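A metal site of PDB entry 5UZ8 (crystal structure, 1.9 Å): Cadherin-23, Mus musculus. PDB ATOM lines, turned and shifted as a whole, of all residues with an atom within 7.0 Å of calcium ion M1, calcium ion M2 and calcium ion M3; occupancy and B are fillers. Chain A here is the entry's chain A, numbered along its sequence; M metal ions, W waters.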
ATOM      1  N   GLU A  21      22.394  -6.456   7.438  1.00  0.00           N
ATOM      2  CA  GLU A  21      22.889  -5.080   7.549  1.00  0.00           C
ATOM      3  C   GLU A  21      22.393  -4.443   8.845  1.00  0.00           C
ATOM      4  O   GLU A  21      21.316  -4.782   9.347  1.00  0.00           O
ATOM      5  CB  GLU A  21      22.508  -4.238   6.336  1.00  0.00           C
ATOM      6  CG  GLU A  21      21.024  -3.958   6.218  1.00  0.00           C
ATOM      7  CD  GLU A  21      20.709  -2.875   5.211  1.00  0.00           C
ATOM      8  OE1 GLU A  21      19.646  -2.982   4.537  1.00  0.00           O
ATOM      9  OE2 GLU A  21      21.495  -1.915   5.124  1.00  0.00           O
ATOM     10  N   GLY A  22      23.213  -3.588   9.433  1.00  0.00           N
ATOM     11  CA  GLY A  22      22.889  -2.927  10.675  1.00  0.00           C
ATOM     12  C   GLY A  22      23.232  -3.679  11.939  1.00  0.00           C
ATOM     13  O   GLY A  22      22.988  -3.160  13.034  1.00  0.00           O
ATOM     14  N   VAL A  74      27.606  -2.368   9.073  1.00  0.00           N
ATOM     15  CA  VAL A  74      27.592  -2.444   7.608  1.00  0.00           C
ATOM     16  C   VAL A  74      26.222  -2.020   7.077  1.00  0.00           C
ATOM     17  O   VAL A  74      25.185  -2.258   7.730  1.00  0.00           O
ATOM     18  CB  VAL A  74      27.979  -3.857   7.132  1.00  0.00           C
ATOM     19  CG1 VAL A  74      26.872  -4.868   7.370  1.00  0.00           C
ATOM     20  CG2 VAL A  74      28.414  -3.846   5.679  1.00  0.00           C
ATOM     21  N   ASP A  75      26.250  -1.398   5.920  1.00  0.00           N
ATOM     22  CA  ASP A  75      25.088  -0.885   5.219  1.00  0.00           C
ATOM     23  C   ASP A  75      24.971  -1.624   3.868  1.00  0.00           C
ATOM     24  O   ASP A  75      25.843  -1.488   3.015  1.00  0.00           O
ATOM     25  CB  ASP A  75      25.294   0.611   4.983  1.00  0.00           C
ATOM     26  CG  ASP A  75      24.107   1.287   4.280  1.00  0.00           C
ATOM     27  OD1 ASP A  75      23.073   0.645   4.006  1.00  0.00           O
ATOM     28  OD2 ASP A  75      24.226   2.484   3.997  1.00  0.00           O
ATOM     29  N   TYR A  76      23.893  -2.373   3.663  1.00  0.00           N
ATOM     30  CA  TYR A  76      23.669  -3.095   2.421  1.00  0.00           C
ATOM     31  C   TYR A  76      23.661  -2.130   1.251  1.00  0.00           C
ATOM     32  O   TYR A  76      24.084  -2.486   0.171  1.00  0.00           O
ATOM     33  CB  TYR A  76      22.345  -3.883   2.454  1.00  0.00           C
ATOM     34  CG  TYR A  76      22.129  -4.701   1.212  1.00  0.00           C
ATOM     35  CD1 TYR A  76      22.731  -5.982   1.068  1.00  0.00           C
ATOM     36  CD2 TYR A  76      21.372  -4.216   0.146  1.00  0.00           C
ATOM     37  CE1 TYR A  76      22.539  -6.721  -0.081  1.00  0.00           C
ATOM     38  CE2 TYR A  76      21.181  -4.971  -0.977  1.00  0.00           C
ATOM     39  CZ  TYR A  76      21.771  -6.195  -1.089  1.00  0.00           C
ATOM     40  OH  TYR A  76      21.575  -6.917  -2.235  1.00  0.00           O
ATOM     41  N   GLU A  77      23.175  -0.913   1.461  1.00  0.00           N
ATOM     42  CA  GLU A  77      23.155   0.061   0.390  1.00  0.00           C
ATOM     43  C   GLU A  77      24.567   0.522  -0.045  1.00  0.00           C
ATOM     44  O   GLU A  77      24.684   1.142  -1.085  1.00  0.00           O
ATOM     45  CB  GLU A  77      22.230   1.230   0.722  1.00  0.00           C
ATOM     46  CG  GLU A  77      20.748   0.916   0.570  1.00  0.00           C
ATOM     47  CD  GLU A  77      20.197  -0.152   1.524  1.00  0.00           C
ATOM     48  OE1 GLU A  77      19.698  -1.138   0.988  1.00  0.00           O
ATOM     49  OE2 GLU A  77      20.218  -0.012   2.777  1.00  0.00           O
ATOM     50  N   GLU A  78      25.615   0.166   0.741  1.00  0.00           N
ATOM     51  CA  GLU A  78      27.023   0.465   0.396  1.00  0.00           C
ATOM     52  C   GLU A  78      27.835  -0.797   0.108  1.00  0.00           C
ATOM     53  O   GLU A  78      28.727  -0.762  -0.733  1.00  0.00           O
ATOM     54  CB  GLU A  78      27.700   1.214   1.554  1.00  0.00           C
ATOM     55  CG  GLU A  78      27.113   2.585   1.817  1.00  0.00           C
ATOM     56  CD  GLU A  78      27.221   3.505   0.612  1.00  0.00           C
ATOM     57  OE1 GLU A  78      28.102   3.270  -0.247  1.00  0.00           O
ATOM     58  OE2 GLU A  78      26.425   4.453   0.503  1.00  0.00           O
ATOM     59  N   VAL A 107      22.767  -9.024   4.051  1.00  0.00           N
ATOM     60  CA  VAL A 107      21.345  -9.198   3.763  1.00  0.00           C
ATOM     61  C   VAL A 107      20.661  -7.853   3.920  1.00  0.00           C
ATOM     62  O   VAL A 107      20.823  -7.182   4.944  1.00  0.00           O
ATOM     63  CB  VAL A 107      20.729 -10.187   4.736  1.00  0.00           C
ATOM     64  CG1 VAL A 107      19.224 -10.337   4.508  1.00  0.00           C
ATOM     65  CG2 VAL A 107      21.420 -11.536   4.606  1.00  0.00           C
ATOM     66  N   ASP A 108      19.922  -7.461   2.889  1.00  0.00           N
ATOM     67  CA  ASP A 108      19.169  -6.204   2.890  1.00  0.00           C
ATOM     68  C   ASP A 108      18.048  -6.284   3.920  1.00  0.00           C
ATOM     69  O   ASP A 108      17.309  -7.286   3.997  1.00  0.00           O
ATOM     70  CB  ASP A 108      18.573  -6.025   1.488  1.00  0.00           C
ATOM     71  CG  ASP A 108      17.787  -4.734   1.296  1.00  0.00           C
ATOM     72  OD1 ASP A 108      18.169  -3.663   1.850  1.00  0.00           O
ATOM     73  OD2 ASP A 108      16.819  -4.783   0.490  1.00  0.00           O
ATOM     74  N   ILE A 109      17.878  -5.211   4.680  1.00  0.00           N
ATOM     75  CA  ILE A 109      16.663  -4.994   5.486  1.00  0.00           C
ATOM     76  C   ILE A 109      15.932  -3.767   4.958  1.00  0.00           C
ATOM     77  O   ILE A 109      16.499  -2.942   4.232  1.00  0.00           O
ATOM     78  CB  ILE A 109      16.954  -4.849   7.011  1.00  0.00           C
ATOM     79  CG1 ILE A 109      17.543  -3.480   7.341  1.00  0.00           C
ATOM     80  CG2 ILE A 109      17.846  -5.987   7.513  1.00  0.00           C
ATOM     81  CD1 ILE A 109      17.912  -3.265   8.805  1.00  0.00           C
ATOM     82  N   ASN A 110      14.658  -3.640   5.304  1.00  0.00           N
ATOM     83  CA  ASN A 110      13.852  -2.567   4.803  1.00  0.00           C
ATOM     84  C   ASN A 110      14.022  -1.322   5.657  1.00  0.00           C
ATOM     85  O   ASN A 110      13.131  -0.936   6.429  1.00  0.00           O
ATOM     86  CB  ASN A 110      12.373  -2.976   4.711  1.00  0.00           C
ATOM     87  CG  ASN A 110      11.539  -1.960   3.960  1.00  0.00           C
ATOM     88  OD1 ASN A 110      12.072  -1.217   3.151  1.00  0.00           O
ATOM     89  ND2 ASN A 110      10.244  -1.928   4.211  1.00  0.00           N
ATOM     90  N   ASP A 111      15.182  -0.677   5.483  1.00  0.00           N
ATOM     91  CA  ASP A 111      15.556   0.503   6.280  1.00  0.00           C
ATOM     92  C   ASP A 111      15.488   1.837   5.517  1.00  0.00           C
ATOM     93  O   ASP A 111      15.890   2.869   6.076  1.00  0.00           O
ATOM     94  CB  ASP A 111      16.907   0.295   6.990  1.00  0.00           C
ATOM     95  CG  ASP A 111      18.090   0.041   6.048  1.00  0.00           C
ATOM     96  OD1 ASP A 111      17.919  -0.331   4.860  1.00  0.00           O
ATOM     97  OD2 ASP A 111      19.242   0.118   6.535  1.00  0.00           O
ATOM     98  N   ASN A 112      14.974   1.833   4.299  1.00  0.00           N
ATOM     99  CA  ASN A 112      14.768   3.076   3.565  1.00  0.00           C
ATOM    100  C   ASN A 112      13.288   3.241   3.196  1.00  0.00           C
ATOM    101  O   ASN A 112      12.654   2.300   2.706  1.00  0.00           O
ATOM    102  CB  ASN A 112      15.623   3.132   2.303  1.00  0.00           C
ATOM    103  CG  ASN A 112      17.107   3.287   2.639  1.00  0.00           C
ATOM    104  OD1 ASN A 112      17.586   4.408   2.809  1.00  0.00           O
ATOM    105  ND2 ASN A 112      17.799   2.156   2.830  1.00  0.00           N
ATOM    106  N   ASN A 113      12.771   4.441   3.397  1.00  0.00           N
ATOM    107  CA  ASN A 113      11.407   4.774   3.007  1.00  0.00           C
ATOM    108  C   ASN A 113      11.395   5.155   1.542  1.00  0.00           C
ATOM    109  O   ASN A 113      12.373   5.753   1.076  1.00  0.00           O
ATOM    110  CB  ASN A 113      10.896   5.991   3.774  1.00  0.00           C
ATOM    111  CG  ASN A 113      10.657   5.702   5.246  1.00  0.00           C
ATOM    112  OD1 ASN A 113      11.516   5.190   5.902  1.00  0.00           O
ATOM    113  ND2 ASN A 113       9.473   6.032   5.743  1.00  0.00           N
ATOM    114  N   PRO A 114      10.242   4.963   0.864  1.00  0.00           N
ATOM    115  CA  PRO A 114      10.091   5.654  -0.424  1.00  0.00           C
ATOM    116  C   PRO A 114      10.062   7.144  -0.201  1.00  0.00           C
ATOM    117  O   PRO A 114       9.469   7.617   0.789  1.00  0.00           O
ATOM    118  CB  PRO A 114       8.746   5.153  -0.964  1.00  0.00           C
ATOM    119  CG  PRO A 114       8.334   4.032  -0.109  1.00  0.00           C
ATOM    120  CD  PRO A 114       9.050   4.202   1.236  1.00  0.00           C
ATOM    121  N   ASP A 142      13.079   4.337  -3.855  1.00  0.00           N
ATOM    122  CA  ASP A 142      13.375   3.583  -2.632  1.00  0.00           C
ATOM    123  C   ASP A 142      14.763   2.924  -2.789  1.00  0.00           C
ATOM    124  O   ASP A 142      15.000   2.150  -3.717  1.00  0.00           O
ATOM    125  CB  ASP A 142      12.299   2.559  -2.388  1.00  0.00           C
ATOM    126  CG  ASP A 142      12.377   1.917  -0.995  1.00  0.00           C
ATOM    127  OD1 ASP A 142      13.414   1.284  -0.675  1.00  0.00           O
ATOM    128  OD2 ASP A 142      11.375   1.929  -0.252  1.00  0.00           O
ATOM    129  N   ALA A 143      15.646   3.223  -1.849  1.00  0.00           N
ATOM    130  CA  ALA A 143      17.037   2.772  -1.892  1.00  0.00           C
ATOM    131  C   ALA A 143      17.325   1.317  -1.506  1.00  0.00           C
ATOM    132  O   ALA A 143      18.440   0.860  -1.688  1.00  0.00           O
ATOM    133  CB  ALA A 143      17.886   3.721  -1.027  1.00  0.00           C
ATOM    134  N   ASP A 144      16.324   0.568  -1.032  1.00  0.00           N
ATOM    135  CA  ASP A 144      16.500  -0.848  -0.738  1.00  0.00           C
ATOM    136  C   ASP A 144      16.507  -1.684  -2.030  1.00  0.00           C
ATOM    137  O   ASP A 144      16.635  -1.126  -3.139  1.00  0.00           O
ATOM    138  CB  ASP A 144      15.417  -1.314   0.255  1.00  0.00           C
ATOM    139  CG  ASP A 144      15.501  -0.576   1.570  1.00  0.00           C
ATOM    140  OD1 ASP A 144      16.602  -0.496   2.143  1.00  0.00           O
ATOM    141  OD2 ASP A 144      14.467  -0.022   2.009  1.00  0.00           O
ATOM    142  N   SER A 145      16.396  -2.986  -1.879  1.00  0.00           N
ATOM    143  CA  SER A 145      16.420  -3.928  -2.969  1.00  0.00           C
ATOM    144  C   SER A 145      15.207  -4.875  -2.916  1.00  0.00           C
ATOM    145  O   SER A 145      14.561  -5.047  -1.888  1.00  0.00           O
ATOM    146  CB  SER A 145      17.724  -4.704  -2.952  1.00  0.00           C
ATOM    147  OG  SER A 145      18.817  -3.778  -3.198  1.00  0.00           O
ATOM    148  N   ASN A 147      11.761  -6.684  -2.943  1.00  0.00           N
ATOM    149  CA  ASN A 147      10.407  -6.269  -2.496  1.00  0.00           C
ATOM    150  C   ASN A 147      10.431  -5.027  -1.606  1.00  0.00           C
ATOM    151  O   ASN A 147       9.505  -4.226  -1.660  1.00  0.00           O
ATOM    152  CB  ASN A 147       9.664  -7.382  -1.757  1.00  0.00           C
ATOM    153  CG  ASN A 147       8.181  -7.334  -2.016  1.00  0.00           C
ATOM    154  OD1 ASN A 147       7.777  -7.568  -3.159  1.00  0.00           O
ATOM    155  ND2 ASN A 147       7.365  -7.017  -1.008  1.00  0.00           N
ATOM    156  N   PHE A 148      11.499  -4.865  -0.839  1.00  0.00           N
ATOM    157  CA  PHE A 148      11.664  -3.716   0.012  1.00  0.00           C
ATOM    158  C   PHE A 148      11.782  -2.390  -0.716  1.00  0.00           C
ATOM    159  O   PHE A 148      11.672  -1.322  -0.088  1.00  0.00           O
ATOM    160  CB  PHE A 148      12.896  -3.937   0.903  1.00  0.00           C
ATOM    161  CG  PHE A 148      12.794  -5.079   1.856  1.00  0.00           C
ATOM    162  CD1 PHE A 148      11.559  -5.580   2.302  1.00  0.00           C
ATOM    163  CD2 PHE A 148      13.945  -5.598   2.413  1.00  0.00           C
ATOM    164  CE1 PHE A 148      11.498  -6.601   3.232  1.00  0.00           C
ATOM    165  CE2 PHE A 148      13.892  -6.607   3.357  1.00  0.00           C
ATOM    166  CZ  PHE A 148      12.663  -7.125   3.770  1.00  0.00           C
ATOM    167  N   ALA A 149      12.015  -2.432  -2.032  1.00  0.00           N
ATOM    168  CA  ALA A 149      12.103  -1.197  -2.853  1.00  0.00           C
ATOM    169  C   ALA A 149      10.981  -1.085  -3.909  1.00  0.00           C
ATOM    170  O   ALA A 149      11.006  -0.152  -4.732  1.00  0.00           O
ATOM    171  CB  ALA A 149      13.474  -1.139  -3.536  1.00  0.00           C
ATOM    172  N   LEU A 150      10.022  -2.019  -3.880  1.00  0.00           N
ATOM    173  CA  LEU A 150       8.854  -1.926  -4.722  1.00  0.00           C
ATOM    174  C   LEU A 150       7.869  -0.995  -4.047  1.00  0.00           C
ATOM    175  O   LEU A 150       7.672  -1.094  -2.839  1.00  0.00           O
ATOM    176  CB  LEU A 150       8.201  -3.272  -4.960  1.00  0.00           C
ATOM    177  CG  LEU A 150       9.054  -4.275  -5.722  1.00  0.00           C
ATOM    178  CD1 LEU A 150       8.255  -5.546  -5.988  1.00  0.00           C
ATOM    179  CD2 LEU A 150       9.500  -3.648  -7.053  1.00  0.00           C
ATOM    180  N   ASP A 193       6.186   1.016   0.515  1.00  0.00           N
ATOM    181  CA  ASP A 193       7.046  -0.021  -0.026  1.00  0.00           C
ATOM    182  C   ASP A 193       6.601  -1.405   0.422  1.00  0.00           C
ATOM    183  O   ASP A 193       5.593  -1.541   1.117  1.00  0.00           O
ATOM    184  CB  ASP A 193       8.529   0.295   0.281  1.00  0.00           C
ATOM    185  CG  ASP A 193       8.882   0.105   1.740  1.00  0.00           C
ATOM    186  OD1 ASP A 193       8.112  -0.526   2.504  1.00  0.00           O
ATOM    187  OD2 ASP A 193       9.983   0.573   2.099  1.00  0.00           O
ATOM    188  N   ASN A 194       7.351  -2.433   0.026  1.00  0.00           N
ATOM    189  CA  ASN A 194       7.248  -3.789   0.541  1.00  0.00           C
ATOM    190  C   ASN A 194       5.835  -4.391   0.438  1.00  0.00           C
ATOM    191  O   ASN A 194       5.239  -4.810   1.436  1.00  0.00           O
ATOM    192  CB  ASN A 194       7.806  -3.856   2.004  1.00  0.00           C
ATOM    193  CG  ASN A 194       8.038  -5.277   2.496  1.00  0.00           C
ATOM    194  OD1 ASN A 194       8.152  -6.235   1.734  1.00  0.00           O
ATOM    195  ND2 ASN A 194       8.125  -5.410   3.843  1.00  0.00           N
ATOM    196  N   ASN A 201       6.204  -3.912   8.624  1.00  0.00           N
ATOM    197  CA  ASN A 201       7.479  -3.958   7.870  1.00  0.00           C
ATOM    198  C   ASN A 201       7.335  -3.178   6.562  1.00  0.00           C
ATOM    199  O   ASN A 201       8.174  -3.296   5.706  1.00  0.00           O
ATOM    200  CB  ASN A 201       7.999  -5.440   7.639  1.00  0.00           C
ATOM    201  CG  ASN A 201       9.544  -5.554   7.287  1.00  0.00           C
ATOM    202  OD1 ASN A 201      10.396  -4.742   7.664  1.00  0.00           O
ATOM    203  ND2 ASN A 201       9.876  -6.617   6.577  1.00  0.00           N
ATOM    204  N   ARG A 203       7.210   0.695   4.897  1.00  0.00           N
ATOM    205  CA  ARG A 203       7.540   2.088   5.109  1.00  0.00           C
ATOM    206  C   ARG A 203       6.850   2.934   4.052  1.00  0.00           C
ATOM    207  O   ARG A 203       6.550   2.481   2.951  1.00  0.00           O
ATOM    208  CB  ARG A 203       9.062   2.295   5.010  1.00  0.00           C
ATOM    209  CG  ARG A 203       9.844   1.751   6.166  1.00  0.00           C
ATOM    210  CD  ARG A 203      11.346   1.856   5.948  1.00  0.00           C
ATOM    211  NE  ARG A 203      12.100   1.513   7.159  1.00  0.00           N
ATOM    212  CZ  ARG A 203      12.362   2.327   8.177  1.00  0.00           C
ATOM    213  NH1 ARG A 203      13.076   1.884   9.193  1.00  0.00           N
ATOM    214  NH2 ARG A 203      11.968   3.591   8.180  1.00  0.00           N
HETATM  215 CA    CA M   1      12.198   0.436   1.444  1.00  0.00          CA
HETATM  216 CA    CA M   2      18.322  -1.767   3.028  1.00  0.00          CA
HETATM  217 CA    CA M   3      20.910   0.417   4.909  1.00  0.00          CA
HETATM  218  O   HOH W   1      20.242   2.644   4.474  1.00  0.00           O
HETATM  219  O   HOH W   2      22.170   1.388   6.770  1.00  0.00           O
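OD2 of Asp 108 is in hydrogen-bond range of N of Ser 145.
The side-chain carboxylate (OE2) of Glu 77 lies close to the side-chain amide nitrogen (ND2) of Asn 112, at 3.2 Å.
OD1 of Asp 111 sits close to ND2 of Asn 112 (3.2 Å).
The side-chain carboxylate (OD1) of Asp 193 sits at hydrogen-bond distance from the backbone NH (N) of Arg 203, at 2.8 Å.
The side-chain carboxylate (OE2) of Glu 21 lies close to the backbone NH (N) of Tyr 76, at 2.8 Å.
The backbone NH (N) of Glu 21 lies within hydrogen-bond range of the backbone carbonyl oxygen (O) of Val 107.
The backbone carbonyl oxygen (O) of Asn 110 is in hydrogen-bond range of the guanidinium group (NE) of Arg 203, 2.8 Å away.
The side-chain amide nitrogen of Asn 110 lies within hydrogen-bond range of the backbone carbonyl oxygen of Asn 201 (2.9 Å).
Within 4 Å of calcium ion M1: Asn 110, Asn 112, Asp 142, Asp 144, Phe 148 and Asp 193.
Within 4 Å of calcium ion M2: Glu 21, Glu 77, Asp 108, Ile 109, Asp 111, Asn 112 and Asp 144.
Along chain A the residues within 4 Å of calcium ion M2 span positions 21 to 144.
Four residues have an atom within 4 Å of calcium ion M3: Glu 21, Asp 75, Glu 77 and Asp 111.
The nearest printed residue that does not touch calcium ion M3 is Asn 112 (4.1 Å).
Calcium ion M1 is bound by the backbone carbonyl oxygen (O) of Asn 112 (2.3 Å), the side-chain carboxylate (OD2) of Asp 193 (2.3 Å), the side-chain amide oxygen (OD1) of Asn 110 (2.4 Å), the side-chain carboxylate (OD2) of Asp 144 (2.4 Å), the backbone carbonyl oxygen (O) of Phe 148 (2.4 Å), the side-chain carboxylate (OD2) of Asp 142 (2.4 Å) and the side-chain carboxylate (OD1) of Asp 142 (2.6 Å).
Calcium ion M1 has seven donor atoms within binding distance.
Calcium ion M2 is bound by the side-chain carboxylate (OD1) of Asp 108, the side-chain carboxylate (OD1) of Asp 144, the side-chain carboxylate (OE1) of Glu 21, the side-chain carboxylate (OD1) of Asp 111, the backbone carbonyl oxygen (O) of Ile 109, the side-chain carboxylate (OE1) of Glu 77 and the side-chain carboxylate (OE2) of Glu 77.
OE2 of Glu 77 binds calcium ion M3, 2.3 Å away.
OD2 of Asp 111 binds calcium ion M3 (2.3 Å).
Calcium ion M3 is bound by the side-chain carboxylate (OD1) of Asp 75 (2.4 Å).
Water W1 is bound to calcium ion M3, at 2.4 Å.
OE2 of Glu 21 is bound to calcium ion M3.
Calcium ion M3 is bound by water W2, at 2.4 Å.
Slightly farther from calcium ion M3 lies the side-chain carboxylate (OD1) of Asp 111 (3.1 Å).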
